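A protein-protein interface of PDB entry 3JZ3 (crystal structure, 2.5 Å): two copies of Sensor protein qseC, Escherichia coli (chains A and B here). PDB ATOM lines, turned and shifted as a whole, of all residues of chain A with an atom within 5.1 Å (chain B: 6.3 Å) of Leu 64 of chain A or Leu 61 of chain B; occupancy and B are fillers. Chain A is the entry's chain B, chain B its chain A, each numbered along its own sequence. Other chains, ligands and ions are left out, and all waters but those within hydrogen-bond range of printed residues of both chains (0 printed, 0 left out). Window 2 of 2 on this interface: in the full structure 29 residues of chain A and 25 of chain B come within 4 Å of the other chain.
The backbone carbonyl oxygen (O) of Leu 58 of chain B is in hydrogen-bond range of the side-chain hydroxyl (OG) of Ser 62 of chain B, at 3.1 Å. The side-chain hydroxyl of Ser 62 of chain B sits at hydrogen-bond distance from the backbone carbonyl oxygen of Leu 59 of chain B, 2.8 Å away. The backbone carbonyl oxygen (O) of Leu 59 of chain A is in hydrogen-bond range of the side-chain hydroxyl (OG) of Ser 62 of chain A.
CB of Leu 61 of chain A touches CB of Ser 62 of chain B, at 3.7 Å. Leu 64 of chain B touches Leu 61 of chain A (CD1 to CD1, 3.9 Å). Ser 62 of chain A touches Leu 61 of chain B. Ser 62 of chain A touches Ser 62 of chain B (CB to N, 3.98 Å). Leu 61 of chain B touches Leu 64 of chain A. Leu 70 of chain A touches Gln 57 of chain B (CA to OE1, 3.4 Å).
Of chain B, only Leu 61 comes within 4 Å of Leu 64 of chain A. Leu 61 of chain B touches just these residues of chain A: Ser 62 and Leu 64. Printed residues of chain B within 4 Å of Leu 70 of chain A: Gln 57 (3.4 Å). Of the printed residues of chain A, Ser 62 of chain B touches Leu 61 (3.7 Å) and Ser 62 (3.98 Å). Of the printed residues of chain A, Gln 57 of chain B touches Leu 70 (3.4 Å). Printed residues of chain B within 4 Å of Ser 62 of chain A: Leu 61 (3.5 Å) and Ser 62 (3.98 Å).
Leu 61 of chain A touches Ser 62 of chain B, and with the chains exchanged Ser 62 of chain A touches Leu 61 of chain B. Leu 61 of chain A touches Leu 64 of chain B, and with the chains exchanged Leu 64 of chain A touches Leu 61 of chain B. Ser 62 of chain A touches its own counterpart, Ser 62 of chain B.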
ATOM      1  N   LEU A  59      18.434   1.773   3.831  1.00  0.00           N
ATOM      2  CA  LEU A  59      18.854   0.406   3.510  1.00  0.00           C
ATOM      3  C   LEU A  59      20.317   0.175   3.873  1.00  0.00           C
ATOM      4  O   LEU A  59      20.656  -0.833   4.499  1.00  0.00           O
ATOM      5  CB  LEU A  59      18.639   0.090   2.025  1.00  0.00           C
ATOM      6  CG  LEU A  59      17.273  -0.402   1.536  1.00  0.00           C
ATOM      7  CD1 LEU A  59      17.296  -0.499   0.025  1.00  0.00           C
ATOM      8  CD2 LEU A  59      16.895  -1.745   2.148  1.00  0.00           C
ATOM      9  N   LEU A  61      22.306   2.034   5.964  1.00  0.00           N
ATOM     10  CA  LEU A  61      22.546   2.186   7.403  1.00  0.00           C
ATOM     11  C   LEU A  61      22.079   0.977   8.202  1.00  0.00           C
ATOM     12  O   LEU A  61      22.721   0.593   9.181  1.00  0.00           O
ATOM     13  CB  LEU A  61      21.887   3.460   7.945  1.00  0.00           C
ATOM     14  CG  LEU A  61      22.327   4.809   7.371  1.00  0.00           C
ATOM     15  CD1 LEU A  61      21.530   5.932   8.005  1.00  0.00           C
ATOM     16  CD2 LEU A  61      23.818   5.034   7.560  1.00  0.00           C
ATOM     17  N   SER A  62      20.968   0.381   7.775  1.00  0.00           N
ATOM     18  CA  SER A  62      20.424  -0.821   8.412  1.00  0.00           C
ATOM     19  C   SER A  62      21.224  -2.078   8.057  1.00  0.00           C
ATOM     20  O   SER A  62      21.007  -3.142   8.643  1.00  0.00           O
ATOM     21  CB  SER A  62      18.959  -1.008   8.017  1.00  0.00           C
ATOM     22  OG  SER A  62      18.826  -1.117   6.611  1.00  0.00           O
ATOM     23  N   ARG A  63      22.154  -1.931   7.109  1.00  0.00           N
ATOM     24  CA  ARG A  63      22.944  -3.035   6.533  1.00  0.00           C
ATOM     25  C   ARG A  63      22.140  -4.334   6.380  1.00  0.00           C
ATOM     26  O   ARG A  63      22.483  -5.382   6.937  1.00  0.00           O
ATOM     27  CB  ARG A  63      24.290  -3.232   7.262  1.00  0.00           C
ATOM     28  CG  ARG A  63      24.223  -3.529   8.763  1.00  0.00           C
ATOM     29  CD  ARG A  63      25.589  -3.381   9.441  1.00  0.00           C
ATOM     30  NE  ARG A  63      26.656  -4.123   8.763  1.00  0.00           N
ATOM     31  CZ  ARG A  63      27.680  -3.566   8.118  1.00  0.00           C
ATOM     32  NH1 ARG A  63      27.808  -2.246   8.056  1.00  0.00           N
ATOM     33  NH2 ARG A  63      28.590  -4.335   7.539  1.00  0.00           N
ATOM     34  N   LEU A  64      21.064  -4.229   5.607  1.00  0.00           N
ATOM     35  CA  LEU A  64      20.102  -5.305   5.435  1.00  0.00           C
ATOM     36  C   LEU A  64      20.652  -6.402   4.535  1.00  0.00           C
ATOM     37  O   LEU A  64      20.991  -6.158   3.375  1.00  0.00           O
ATOM     38  CB  LEU A  64      18.804  -4.740   4.863  1.00  0.00           C
ATOM     39  CG  LEU A  64      17.495  -5.460   5.179  1.00  0.00           C
ATOM     40  CD1 LEU A  64      17.292  -5.634   6.682  1.00  0.00           C
ATOM     41  CD2 LEU A  64      16.351  -4.674   4.572  1.00  0.00           C
ATOM     42  N   ASP A  65      20.732  -7.610   5.087  1.00  0.00           N
ATOM     43  CA  ASP A  65      21.354  -8.751   4.412  1.00  0.00           C
ATOM     44  C   ASP A  65      20.382  -9.542   3.531  1.00  0.00           C
ATOM     45  O   ASP A  65      20.692  -9.841   2.373  1.00  0.00           O
ATOM     46  CB  ASP A  65      22.033  -9.679   5.436  1.00  0.00           C
ATOM     47  CG  ASP A  65      21.124 -10.031   6.613  1.00  0.00           C
ATOM     48  OD1 ASP A  65      20.781  -9.123   7.405  1.00  0.00           O
ATOM     49  OD2 ASP A  65      20.762 -11.219   6.751  1.00  0.00           O
ATOM     50  N   SER A  66      19.215  -9.872   4.079  1.00  0.00           N
ATOM     51  CA  SER A  66      18.238 -10.703   3.381  1.00  0.00           C
ATOM     52  C   SER A  66      16.810 -10.193   3.567  1.00  0.00           C
ATOM     53  O   SER A  66      16.572  -9.226   4.291  1.00  0.00           O
ATOM     54  CB  SER A  66      18.343 -12.153   3.864  1.00  0.00           C
ATOM     55  OG  SER A  66      17.886 -12.275   5.200  1.00  0.00           O
ATOM     56  N   LEU A  70      12.146  -8.714   6.775  1.00  0.00           N
ATOM     57  CA  LEU A  70      11.474  -7.534   6.232  1.00  0.00           C
ATOM     58  C   LEU A  70       9.963  -7.658   6.274  1.00  0.00           C
ATOM     59  O   LEU A  70       9.414  -8.726   6.003  1.00  0.00           O
ATOM     60  CB  LEU A  70      11.905  -7.267   4.789  1.00  0.00           C
ATOM     61  CG  LEU A  70      12.980  -6.225   4.501  1.00  0.00           C
ATOM     62  CD1 LEU A  70      13.219  -6.165   3.007  1.00  0.00           C
ATOM     63  CD2 LEU A  70      12.590  -4.855   5.040  1.00  0.00           C
ATOM     64  N   LEU A 193      19.714  -7.513  -2.707  1.00  0.00           N
ATOM     65  CA  LEU A 193      18.893  -7.942  -1.580  1.00  0.00           C
ATOM     66  C   LEU A 193      17.890  -9.026  -1.995  1.00  0.00           C
ATOM     67  O   LEU A 193      17.587  -9.926  -1.212  1.00  0.00           O
ATOM     68  CB  LEU A 193      18.174  -6.734  -0.969  1.00  0.00           C
ATOM     69  CG  LEU A 193      17.229  -6.904   0.223  1.00  0.00           C
ATOM     70  CD1 LEU A 193      17.981  -7.301   1.486  1.00  0.00           C
ATOM     71  CD2 LEU A 193      16.455  -5.620   0.451  1.00  0.00           C
ATOM     72  N   ASP B  56       9.194   2.414   8.956  1.00  0.00           N
ATOM     73  CA  ASP B  56       9.373   2.230  10.394  1.00  0.00           C
ATOM     74  C   ASP B  56      10.483   1.226  10.695  1.00  0.00           C
ATOM     75  O   ASP B  56      11.371   1.503  11.500  1.00  0.00           O
ATOM     76  CB  ASP B  56       8.066   1.778  11.047  1.00  0.00           C
ATOM     77  CG  ASP B  56       8.176   1.663  12.557  1.00  0.00           C
ATOM     78  OD1 ASP B  56       8.834   2.523  13.179  1.00  0.00           O
ATOM     79  OD2 ASP B  56       7.599   0.711  13.123  1.00  0.00           O
ATOM     80  N   GLN B  57      10.427   0.068  10.038  1.00  0.00           N
ATOM     81  CA  GLN B  57      11.432  -0.974  10.219  1.00  0.00           C
ATOM     82  C   GLN B  57      12.820  -0.521   9.764  1.00  0.00           C
ATOM     83  O   GLN B  57      13.817  -0.811  10.428  1.00  0.00           O
ATOM     84  CB  GLN B  57      11.025  -2.256   9.494  1.00  0.00           C
ATOM     85  CG  GLN B  57      11.926  -3.444   9.809  1.00  0.00           C
ATOM     86  CD  GLN B  57      11.534  -4.711   9.073  1.00  0.00           C
ATOM     87  OE1 GLN B  57      10.874  -4.668   8.031  1.00  0.00           O
ATOM     88  NE2 GLN B  57      11.949  -5.853   9.611  1.00  0.00           N
ATOM     89  N   LEU B  58      12.888   0.190   8.644  1.00  0.00           N
ATOM     90  CA  LEU B  58      14.167   0.702   8.162  1.00  0.00           C
ATOM     91  C   LEU B  58      14.771   1.754   9.099  1.00  0.00           C
ATOM     92  O   LEU B  58      15.989   1.797   9.279  1.00  0.00           O
ATOM     93  CB  LEU B  58      14.050   1.240   6.734  1.00  0.00           C
ATOM     94  CG  LEU B  58      13.794   0.236   5.597  1.00  0.00           C
ATOM     95  CD1 LEU B  58      13.887   0.933   4.250  1.00  0.00           C
ATOM     96  CD2 LEU B  58      14.747  -0.955   5.640  1.00  0.00           C
ATOM     97  N   LEU B  59      13.918   2.584   9.701  1.00  0.00           N
ATOM     98  CA  LEU B  59      14.356   3.565  10.695  1.00  0.00           C
ATOM     99  C   LEU B  59      14.868   2.899  11.966  1.00  0.00           C
ATOM    100  O   LEU B  59      15.873   3.324  12.534  1.00  0.00           O
ATOM    101  CB  LEU B  59      13.223   4.534  11.049  1.00  0.00           C
ATOM    102  CG  LEU B  59      13.048   5.796  10.201  1.00  0.00           C
ATOM    103  CD1 LEU B  59      11.769   6.505  10.595  1.00  0.00           C
ATOM    104  CD2 LEU B  59      14.240   6.727  10.355  1.00  0.00           C
ATOM    105  N   THR B  60      14.164   1.860  12.402  1.00  0.00           N
ATOM    106  CA  THR B  60      14.519   1.109  13.604  1.00  0.00           C
ATOM    107  C   THR B  60      15.824   0.326  13.431  1.00  0.00           C
ATOM    108  O   THR B  60      16.667   0.313  14.330  1.00  0.00           O
ATOM    109  CB  THR B  60      13.367   0.167  14.017  1.00  0.00           C
ATOM    110  OG1 THR B  60      12.229   0.953  14.399  1.00  0.00           O
ATOM    111  CG2 THR B  60      13.771  -0.731  15.181  1.00  0.00           C
ATOM    112  N   LEU B  61      15.986  -0.309  12.272  1.00  0.00           N
ATOM    113  CA  LEU B  61      17.179  -1.103  11.977  1.00  0.00           C
ATOM    114  C   LEU B  61      18.422  -0.251  11.715  1.00  0.00           C
ATOM    115  O   LEU B  61      19.547  -0.739  11.831  1.00  0.00           O
ATOM    116  CB  LEU B  61      16.927  -2.047  10.800  1.00  0.00           C
ATOM    117  CG  LEU B  61      16.070  -3.289  11.057  1.00  0.00           C
ATOM    118  CD1 LEU B  61      15.673  -3.937   9.743  1.00  0.00           C
ATOM    119  CD2 LEU B  61      16.800  -4.284  11.949  1.00  0.00           C
ATOM    120  N   SER B  62      18.218   1.016  11.358  1.00  0.00           N
ATOM    121  CA  SER B  62      19.330   1.949  11.182  1.00  0.00           C
ATOM    122  C   SER B  62      19.763   2.566  12.517  1.00  0.00           C
ATOM    123  O   SER B  62      20.845   3.154  12.612  1.00  0.00           O
ATOM    124  CB  SER B  62      18.979   3.037  10.162  1.00  0.00           C
ATOM    125  OG  SER B  62      17.909   3.843  10.620  1.00  0.00           O
ATOM    126  N   ARG B  63      18.916   2.411  13.538  1.00  0.00           N
ATOM    127  CA  ARG B  63      19.157   2.942  14.888  1.00  0.00           C
ATOM    128  C   ARG B  63      19.606   4.404  14.837  1.00  0.00           C
ATOM    129  O   ARG B  63      20.571   4.804  15.495  1.00  0.00           O
ATOM    130  CB  ARG B  63      20.165   2.069  15.652  1.00  0.00           C
ATOM    131  N   LEU B  64      18.884   5.190  14.043  1.00  0.00           N
ATOM    132  CA  LEU B  64      19.234   6.575  13.756  1.00  0.00           C
ATOM    133  C   LEU B  64      18.811   7.505  14.890  1.00  0.00           C
ATOM    134  O   LEU B  64      17.709   7.383  15.423  1.00  0.00           O
ATOM    135  CB  LEU B  64      18.583   7.000  12.440  1.00  0.00           C
ATOM    136  CG  LEU B  64      19.109   8.224  11.692  1.00  0.00           C
ATOM    137  CD1 LEU B  64      20.504   7.987  11.121  1.00  0.00           C
ATOM    138  CD2 LEU B  64      18.136   8.562  10.591  1.00  0.00           C
